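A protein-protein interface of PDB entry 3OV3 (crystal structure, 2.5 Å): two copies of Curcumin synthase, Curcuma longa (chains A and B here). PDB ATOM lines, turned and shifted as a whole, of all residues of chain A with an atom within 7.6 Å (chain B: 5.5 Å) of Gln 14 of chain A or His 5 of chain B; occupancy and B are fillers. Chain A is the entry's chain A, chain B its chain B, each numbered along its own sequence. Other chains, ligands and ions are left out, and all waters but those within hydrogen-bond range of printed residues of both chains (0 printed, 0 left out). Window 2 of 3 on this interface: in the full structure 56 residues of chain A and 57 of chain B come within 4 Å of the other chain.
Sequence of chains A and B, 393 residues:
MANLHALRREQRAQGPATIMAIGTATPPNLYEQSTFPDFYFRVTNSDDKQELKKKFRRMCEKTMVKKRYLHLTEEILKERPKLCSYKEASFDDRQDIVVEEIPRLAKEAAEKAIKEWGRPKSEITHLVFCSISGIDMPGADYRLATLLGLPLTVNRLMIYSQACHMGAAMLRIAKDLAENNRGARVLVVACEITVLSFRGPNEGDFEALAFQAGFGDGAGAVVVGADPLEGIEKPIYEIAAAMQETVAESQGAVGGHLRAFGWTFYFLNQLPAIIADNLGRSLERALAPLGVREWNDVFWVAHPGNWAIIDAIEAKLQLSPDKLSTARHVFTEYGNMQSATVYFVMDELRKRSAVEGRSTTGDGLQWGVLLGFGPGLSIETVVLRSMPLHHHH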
ATOM      1  N   ARG A   9      30.330   8.649 -21.560  1.00  0.00           N
ATOM      2  CA  ARG A   9      30.051   9.779 -22.455  1.00  0.00           C
ATOM      3  C   ARG A   9      29.067   9.420 -23.571  1.00  0.00           C
ATOM      4  O   ARG A   9      28.263  10.255 -24.003  1.00  0.00           O
ATOM      5  CB  ARG A   9      31.346  10.340 -23.052  1.00  0.00           C
ATOM      6  CG  ARG A   9      32.278  11.073 -22.057  1.00  0.00           C
ATOM      7  CD  ARG A   9      33.154  12.165 -22.728  1.00  0.00           C
ATOM      8  NE  ARG A   9      33.867  11.681 -23.917  1.00  0.00           N
ATOM      9  CZ  ARG A   9      33.378  11.703 -25.162  1.00  0.00           C
ATOM     10  NH1 ARG A   9      34.103  11.227 -26.169  1.00  0.00           N
ATOM     11  NH2 ARG A   9      32.160  12.188 -25.403  1.00  0.00           N
ATOM     12  N   GLU A  10      29.129   8.168 -24.016  1.00  0.00           N
ATOM     13  CA  GLU A  10      28.286   7.684 -25.109  1.00  0.00           C
ATOM     14  C   GLU A  10      26.854   7.368 -24.674  1.00  0.00           C
ATOM     15  O   GLU A  10      25.899   7.743 -25.352  1.00  0.00           O
ATOM     16  CB  GLU A  10      28.914   6.452 -25.775  1.00  0.00           C
ATOM     17  CG  GLU A  10      30.186   6.746 -26.593  1.00  0.00           C
ATOM     18  CD  GLU A  10      30.321   5.844 -27.819  1.00  0.00           C
ATOM     19  OE1 GLU A  10      29.309   5.644 -28.541  1.00  0.00           O
ATOM     20  OE2 GLU A  10      31.441   5.344 -28.061  1.00  0.00           O
ATOM     21  N   ARG A  12      25.084   8.546 -22.362  1.00  0.00           N
ATOM     22  CA  ARG A  12      24.306   9.651 -21.793  1.00  0.00           C
ATOM     23  C   ARG A  12      23.719  10.639 -22.820  1.00  0.00           C
ATOM     24  O   ARG A  12      24.250  10.783 -23.908  1.00  0.00           O
ATOM     25  CB  ARG A  12      25.060  10.350 -20.646  1.00  0.00           C
ATOM     26  CG  ARG A  12      26.216  11.211 -21.059  1.00  0.00           C
ATOM     27  CD  ARG A  12      26.810  11.911 -19.845  1.00  0.00           C
ATOM     28  NE  ARG A  12      27.860  12.855 -20.227  1.00  0.00           N
ATOM     29  CZ  ARG A  12      28.911  13.166 -19.467  1.00  0.00           C
ATOM     30  NH1 ARG A  12      29.829  14.037 -19.911  1.00  0.00           N
ATOM     31  NH2 ARG A  12      29.047  12.596 -18.266  1.00  0.00           N
ATOM     32  N   ALA A  13      22.616  11.295 -22.468  1.00  0.00           N
ATOM     33  CA  ALA A  13      22.006  12.313 -23.320  1.00  0.00           C
ATOM     34  C   ALA A  13      22.857  13.583 -23.354  1.00  0.00           C
ATOM     35  O   ALA A  13      23.782  13.718 -22.562  1.00  0.00           O
ATOM     36  CB  ALA A  13      20.589  12.625 -22.860  1.00  0.00           C
ATOM     37  N   GLN A  14      22.547  14.506 -24.267  1.00  0.00           N
ATOM     38  CA  GLN A  14      23.360  15.717 -24.448  1.00  0.00           C
ATOM     39  C   GLN A  14      22.740  17.013 -23.930  1.00  0.00           C
ATOM     40  O   GLN A  14      23.455  17.845 -23.388  1.00  0.00           O
ATOM     41  CB  GLN A  14      23.797  15.887 -25.917  1.00  0.00           C
ATOM     42  CG  GLN A  14      24.594  14.691 -26.469  1.00  0.00           C
ATOM     43  CD  GLN A  14      25.907  15.089 -27.126  1.00  0.00           C
ATOM     44  OE1 GLN A  14      26.393  16.226 -26.956  1.00  0.00           O
ATOM     45  NE2 GLN A  14      26.499  14.151 -27.887  1.00  0.00           N
ATOM     46  N   GLY A  15      21.429  17.179 -24.117  1.00  0.00           N
ATOM     47  CA  GLY A  15      20.713  18.413 -23.802  1.00  0.00           C
ATOM     48  C   GLY A  15      19.765  18.242 -22.636  1.00  0.00           C
ATOM     49  O   GLY A  15      19.750  17.189 -22.011  1.00  0.00           O
ATOM     50  N   PRO A  16      18.960  19.274 -22.324  1.00  0.00           N
ATOM     51  CA  PRO A  16      18.090  19.187 -21.135  1.00  0.00           C
ATOM     52  C   PRO A  16      16.841  18.316 -21.337  1.00  0.00           C
ATOM     53  O   PRO A  16      16.328  18.201 -22.456  1.00  0.00           O
ATOM     54  CB  PRO A  16      17.678  20.648 -20.903  1.00  0.00           C
ATOM     55  CG  PRO A  16      17.627  21.236 -22.289  1.00  0.00           C
ATOM     56  CD  PRO A  16      18.805  20.569 -23.021  1.00  0.00           C
ATOM     57  N   ALA A  17      16.356  17.724 -20.248  1.00  0.00           N
ATOM     58  CA  ALA A  17      15.043  17.081 -20.223  1.00  0.00           C
ATOM     59  C   ALA A  17      13.945  18.002 -20.745  1.00  0.00           C
ATOM     60  O   ALA A  17      13.935  19.197 -20.463  1.00  0.00           O
ATOM     61  CB  ALA A  17      14.700  16.628 -18.815  1.00  0.00           C
ATOM     62  N   ALA A 178      15.890  11.126 -17.857  1.00  0.00           N
ATOM     63  CA  ALA A 178      15.960  11.580 -19.236  1.00  0.00           C
ATOM     64  C   ALA A 178      17.362  12.047 -19.628  1.00  0.00           C
ATOM     65  O   ALA A 178      17.838  11.708 -20.705  1.00  0.00           O
ATOM     66  CB  ALA A 178      14.918  12.677 -19.522  1.00  0.00           C
ATOM     67  N   GLU A 179      18.026  12.806 -18.750  1.00  0.00           N
ATOM     68  CA  GLU A 179      19.296  13.454 -19.100  1.00  0.00           C
ATOM     69  C   GLU A 179      20.511  12.536 -19.079  1.00  0.00           C
ATOM     70  O   GLU A 179      21.466  12.752 -19.847  1.00  0.00           O
ATOM     71  CB  GLU A 179      19.548  14.655 -18.200  1.00  0.00           C
ATOM     72  CG  GLU A 179      18.915  15.949 -18.725  1.00  0.00           C
ATOM     73  CD  GLU A 179      18.660  17.000 -17.642  1.00  0.00           C
ATOM     74  OE1 GLU A 179      19.287  16.935 -16.541  1.00  0.00           O
ATOM     75  OE2 GLU A 179      17.819  17.894 -17.908  1.00  0.00           O
ATOM     76  N   ASN A 180      20.485  11.535 -18.193  1.00  0.00           N
ATOM     77  CA  ASN A 180      21.648  10.682 -17.988  1.00  0.00           C
ATOM     78  C   ASN A 180      21.694   9.441 -18.895  1.00  0.00           C
ATOM     79  O   ASN A 180      22.617   8.625 -18.786  1.00  0.00           O
ATOM     80  CB  ASN A 180      21.781  10.259 -16.514  1.00  0.00           C
ATOM     81  CG  ASN A 180      23.170   9.738 -16.194  1.00  0.00           C
ATOM     82  OD1 ASN A 180      24.172  10.424 -16.433  1.00  0.00           O
ATOM     83  ND2 ASN A 180      23.246   8.525 -15.682  1.00  0.00           N
ATOM     84  N   ASN A 181      20.684   9.305 -19.762  1.00  0.00           N
ATOM     85  CA  ASN A 181      20.530   8.134 -20.644  1.00  0.00           C
ATOM     86  C   ASN A 181      20.149   8.518 -22.057  1.00  0.00           C
ATOM     87  O   ASN A 181      19.013   8.884 -22.310  1.00  0.00           O
ATOM     88  CB  ASN A 181      19.464   7.187 -20.086  1.00  0.00           C
ATOM     89  CG  ASN A 181      19.803   6.719 -18.740  1.00  0.00           C
ATOM     90  OD1 ASN A 181      20.725   5.949 -18.581  1.00  0.00           O
ATOM     91  ND2 ASN A 181      19.112   7.231 -17.734  1.00  0.00           N
ATOM     92  N   ARG A 182      21.102   8.412 -22.972  1.00  0.00           N
ATOM     93  CA  ARG A 182      20.873   8.762 -24.377  1.00  0.00           C
ATOM     94  C   ARG A 182      19.652   7.963 -24.847  1.00  0.00           C
ATOM     95  O   ARG A 182      19.591   6.740 -24.612  1.00  0.00           O
ATOM     96  CB  ARG A 182      22.134   8.433 -25.208  1.00  0.00           C
ATOM     97  CG  ARG A 182      22.090   8.798 -26.696  1.00  0.00           C
ATOM     98  CD  ARG A 182      23.395   8.396 -27.463  1.00  0.00           C
ATOM     99  NE  ARG A 182      23.855   6.995 -27.309  1.00  0.00           N
ATOM    100  CZ  ARG A 182      23.107   5.886 -27.474  1.00  0.00           C
ATOM    101  NH1 ARG A 182      21.808   5.963 -27.775  1.00  0.00           N
ATOM    102  NH2 ARG A 182      23.654   4.674 -27.313  1.00  0.00           N
ATOM    103  N   GLY A 183      18.664   8.646 -25.435  1.00  0.00           N
ATOM    104  CA  GLY A 183      17.482   7.973 -25.983  1.00  0.00           C
ATOM    105  C   GLY A 183      16.310   7.689 -25.038  1.00  0.00           C
ATOM    106  O   GLY A 183      15.239   7.285 -25.484  1.00  0.00           O
ATOM    107  N   ALA A 226      15.261  13.969 -23.129  1.00  0.00           N
ATOM    108  CA  ALA A 226      16.282  14.826 -23.706  1.00  0.00           C
ATOM    109  C   ALA A 226      16.447  14.591 -25.240  1.00  0.00           C
ATOM    110  O   ALA A 226      15.936  13.617 -25.781  1.00  0.00           O
ATOM    111  CB  ALA A 226      17.578  14.612 -22.960  1.00  0.00           C
ATOM    112  N   ASP A 227      17.136  15.508 -25.914  1.00  0.00           N
ATOM    113  CA  ASP A 227      17.490  15.402 -27.341  1.00  0.00           C
ATOM    114  C   ASP A 227      16.303  15.157 -28.289  1.00  0.00           C
ATOM    115  O   ASP A 227      16.287  14.188 -29.038  1.00  0.00           O
ATOM    116  CB  ASP A 227      18.602  14.345 -27.585  1.00  0.00           C
ATOM    117  CG  ASP A 227      19.760  14.471 -26.608  1.00  0.00           C
ATOM    118  OD1 ASP A 227      20.254  15.599 -26.400  1.00  0.00           O
ATOM    119  OD2 ASP A 227      20.176  13.438 -26.037  1.00  0.00           O
ATOM    120  N   PRO A 228      15.307  16.042 -28.264  1.00  0.00           N
ATOM    121  CA  PRO A 228      14.119  15.816 -29.129  1.00  0.00           C
ATOM    122  C   PRO A 228      14.450  15.478 -30.614  1.00  0.00           C
ATOM    123  O   PRO A 228      15.307  16.116 -31.215  1.00  0.00           O
ATOM    124  CB  PRO A 228      13.337  17.141 -28.999  1.00  0.00           C
ATOM    125  CG  PRO A 228      14.354  18.153 -28.372  1.00  0.00           C
ATOM    126  CD  PRO A 228      15.224  17.305 -27.511  1.00  0.00           C
ATOM    127  N   GLU A 238      11.225  22.993 -21.256  1.00  0.00           N
ATOM    128  CA  GLU A 238      12.506  22.392 -20.880  1.00  0.00           C
ATOM    129  C   GLU A 238      12.587  22.451 -19.356  1.00  0.00           C
ATOM    130  O   GLU A 238      12.284  23.483 -18.758  1.00  0.00           O
ATOM    131  CB  GLU A 238      13.688  23.123 -21.545  1.00  0.00           C
ATOM    132  CG  GLU A 238      13.673  23.045 -23.111  1.00  0.00           C
ATOM    133  CD  GLU A 238      14.838  23.772 -23.842  1.00  0.00           C
ATOM    134  OE1 GLU A 238      15.491  24.694 -23.278  1.00  0.00           O
ATOM    135  OE2 GLU A 238      15.078  23.422 -25.033  1.00  0.00           O
ATOM    136  N   ASN B   3      23.851  27.640 -24.186  1.00  0.00           N
ATOM    137  CA  ASN B   3      22.878  28.270 -23.238  1.00  0.00           C
ATOM    138  C   ASN B   3      22.490  27.302 -22.120  1.00  0.00           C
ATOM    139  O   ASN B   3      23.084  27.327 -21.037  1.00  0.00           O
ATOM    140  CB  ASN B   3      21.631  28.772 -23.986  1.00  0.00           C
ATOM    141  CG  ASN B   3      20.708  29.617 -23.103  1.00  0.00           C
ATOM    142  OD1 ASN B   3      19.896  29.088 -22.332  1.00  0.00           O
ATOM    143  ND2 ASN B   3      20.822  30.941 -23.231  1.00  0.00           N
ATOM    144  N   LEU B   4      21.486  26.464 -22.397  1.00  0.00           N
ATOM    145  CA  LEU B   4      21.094  25.344 -21.521  1.00  0.00           C
ATOM    146  C   LEU B   4      21.823  24.038 -21.915  1.00  0.00           C
ATOM    147  O   LEU B   4      21.816  23.056 -21.159  1.00  0.00           O
ATOM    148  CB  LEU B   4      19.562  25.174 -21.501  1.00  0.00           C
ATOM    149  CG  LEU B   4      18.849  24.269 -20.483  1.00  0.00           C
ATOM    150  CD1 LEU B   4      19.471  24.317 -19.065  1.00  0.00           C
ATOM    151  CD2 LEU B   4      17.348  24.601 -20.452  1.00  0.00           C
ATOM    152  N   HIS B   5      22.446  24.046 -23.099  1.00  0.00           N
ATOM    153  CA  HIS B   5      23.458  23.052 -23.477  1.00  0.00           C
ATOM    154  C   HIS B   5      24.770  23.365 -22.752  1.00  0.00           C
ATOM    155  O   HIS B   5      25.427  22.459 -22.225  1.00  0.00           O
ATOM    156  CB  HIS B   5      23.665  22.998 -25.003  1.00  0.00           C
ATOM    157  CG  HIS B   5      22.834  21.952 -25.685  1.00  0.00           C
ATOM    158  ND1 HIS B   5      21.534  22.176 -26.090  1.00  0.00           N
ATOM    159  CD2 HIS B   5      23.113  20.668 -26.017  1.00  0.00           C
ATOM    160  CE1 HIS B   5      21.047  21.077 -26.639  1.00  0.00           C
ATOM    161  NE2 HIS B   5      21.987  20.148 -26.612  1.00  0.00           N
ATOM    162  N   ALA B   6      25.126  24.651 -22.720  1.00  0.00           N
ATOM    163  CA  ALA B   6      26.242  25.138 -21.914  1.00  0.00           C
ATOM    164  C   ALA B   6      26.062  24.767 -20.434  1.00  0.00           C
ATOM    165  O   ALA B   6      26.843  23.980 -19.891  1.00  0.00           O
ATOM    166  CB  ALA B   6      26.410  26.648 -22.086  1.00  0.00           C
ATOM    167  N   LEU B   7      25.022  25.307 -19.798  1.00  0.00           N
ATOM    168  CA  LEU B   7      24.743  25.028 -18.381  1.00  0.00           C
ATOM    169  C   LEU B   7      24.656  23.528 -18.090  1.00  0.00           C
ATOM    170  O   LEU B   7      25.169  23.059 -17.073  1.00  0.00           O
ATOM    171  CB  LEU B   7      23.467  25.740 -17.893  1.00  0.00           C
ATOM    172  CG  LEU B   7      23.481  26.319 -16.461  1.00  0.00           C
ATOM    173  CD1 LEU B   7      23.731  27.859 -16.509  1.00  0.00           C
ATOM    174  CD2 LEU B   7      22.191  25.981 -15.699  1.00  0.00           C
ATOM    175  N   ARG B   8      24.011  22.786 -18.990  1.00  0.00           N
ATOM    176  CA  ARG B   8      23.976  21.333 -18.917  1.00  0.00           C
ATOM    177  C   ARG B   8      25.355  20.730 -18.638  1.00  0.00           C
ATOM    178  O   ARG B   8      25.482  19.891 -17.757  1.00  0.00           O
ATOM    179  CB  ARG B   8      23.367  20.747 -20.186  1.00  0.00           C
ATOM    180  CG  ARG B   8      22.922  19.297 -20.081  1.00  0.00           C
ATOM    181  CD  ARG B   8      21.557  19.118 -19.402  1.00  0.00           C
ATOM    182  NE  ARG B   8      21.650  19.022 -17.947  1.00  0.00           N
ATOM    183  CZ  ARG B   8      22.158  17.985 -17.274  1.00  0.00           C
ATOM    184  NH1 ARG B   8      22.655  16.918 -17.911  1.00  0.00           N
ATOM    185  NH2 ARG B   8      22.181  18.013 -15.944  1.00  0.00           N
ATOM    186  N   ARG B   9      26.388  21.173 -19.360  1.00  0.00           N
ATOM    187  CA  ARG B   9      27.764  20.682 -19.140  1.00  0.00           C
ATOM    188  C   ARG B   9      28.319  21.018 -17.751  1.00  0.00           C
ATOM    189  O   ARG B   9      29.100  20.254 -17.185  1.00  0.00           O
ATOM    190  CB  ARG B   9      28.729  21.194 -20.226  1.00  0.00           C
ATOM    191  CG  ARG B   9      28.934  20.232 -21.411  1.00  0.00           C
ATOM    192  CD  ARG B   9      30.010  20.711 -22.397  1.00  0.00           C
ATOM    193  NE  ARG B   9      29.788  22.100 -22.825  1.00  0.00           N
ATOM    194  CZ  ARG B   9      29.182  22.473 -23.956  1.00  0.00           C
ATOM    195  NH1 ARG B   9      28.724  21.564 -24.812  1.00  0.00           N
ATOM    196  NH2 ARG B   9      29.035  23.763 -24.234  1.00  0.00           N
ATOM    197  N   ARG B  12      26.372  18.612 -14.860  1.00  0.00           N
ATOM    198  CA  ARG B  12      26.455  17.146 -14.861  1.00  0.00           C
ATOM    199  C   ARG B  12      27.808  16.636 -14.321  1.00  0.00           C
ATOM    200  O   ARG B  12      28.823  17.362 -14.349  1.00  0.00           O
ATOM    201  CB  ARG B  12      26.111  16.570 -16.250  1.00  0.00           C
ATOM    202  CG  ARG B  12      27.196  16.755 -17.306  1.00  0.00           C
ATOM    203  CD  ARG B  12      26.697  16.609 -18.741  1.00  0.00           C
ATOM    204  NE  ARG B  12      25.841  15.439 -18.916  1.00  0.00           N
ATOM    205  CZ  ARG B  12      24.955  15.275 -19.906  1.00  0.00           C
ATOM    206  NH1 ARG B  12      24.796  16.218 -20.852  1.00  0.00           N
ATOM    207  NH2 ARG B  12      24.222  14.161 -19.944  1.00  0.00           N
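Arg 12 of chain B touches its own counterpart, Arg 12 of chain A. Positions printed for both chains: 9 and 12. Of the 12 pairs that touch across the chains among the printed residues, 1 has its exchanged pair printed and touching as well.
The side-chain carboxylate (OD1) of Asp 227 of chain A is in hydrogen-bond range of the backbone NH (N) of Gly 15 of chain A (3.0 Å). N of Ala 13 of chain A sits close to O of Glu 179 of chain A (3.2 Å). The backbone NH (N) of Ala 17 of chain A lies within hydrogen-bond range of the side-chain carboxylate (OE2) of Glu 179 of chain A (2.8 Å). The side-chain carboxylate (OD2) of Asp 227 of chain A is in hydrogen-bond range of the backbone NH (N) of Gln 14 of chain A (3.1 Å).
OE1 of Glu 179 of chain A is in salt-bridge range of NH2 of Arg 8 of chain B (3.1 Å). The backbone carbonyl oxygen (O) of Glu 179 of chain A is in hydrogen-bond range of the guanidinium group (NH2) of Arg 12 of chain B, at 3.1 Å. O of Ala 13 of chain A is in hydrogen-bond range of NH2 of Arg 12 of chain B, 2.7 Å away. The backbone carbonyl oxygen (O) of Gln 14 of chain A is in hydrogen-bond range of the guanidinium group (NH1) of Arg 12 of chain B.
Of the 8 printed residues of chain B, 4 touch a printed residue of chain A. Printed residues of chain B that touch a printed residue of chain A: Leu 4, His 5, Arg 8 and Arg 12. Hydrophobic or aromatic side chains of chain B within 4 Å of the printed part of chain A: Leu 4 and His 5. Of the 18 printed residues of chain A, 7 touch a printed residue of chain B. Hydrophobic or aromatic side chains of chain A that line the printed part of chain B: Pro 16. Along chain A the printed residues that touch a printed residue of chain B span positions 12 to 238. Among the printed residues, Asp or Glu carboxylates within 4 Å of a Lys or Arg side-chain nitrogen of the other chain: Glu 179 of chain A with Arg 8 of chain B.
Gln 14 of chain A touches just these residues of chain B: His 5 (3.9 Å), Arg 8 (3.7 Å) and Arg 12 (3.3 Å). Printed residues of chain B within 4 Å of Pro 16 of chain A: Leu 4 and Arg 8. Printed residues of chain A within 4 Å of Leu 4 of chain B: Pro 16 and Glu 238. Of chain A, only Gln 14 (3.9 Å) and Gly 15 (3.5 Å) come within 4 Å of His 5 of chain B. Of the printed residues of chain A, Arg 12 of chain B touches Arg 12, Ala 13, Gln 14 and Glu 179. The nearest printed residue of chain B that does not touch Gln 14 of chain A is Leu 4 of chain B (5.9 Å). The nearest printed residue of chain B that does not touch Glu 238 of chain A is Asn 3 of chain B (6.3 Å).
Among the printed residues, pairs that only touch across the chains: Glu 238 of chain A with Leu 4 of chain B, Arg 12 of chain A with Arg 12 of chain B, Gly 15 of chain A with His 5 of chain B, Gln 14 of chain A with Arg 8 of chain B, Gly 15 of chain A with Arg 8 of chain B, Pro 16 of chain A with Leu 4 of chain B, Gln 14 of chain A with His 5 of chain B and Pro 16 of chain A with Arg 8 of chain B.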
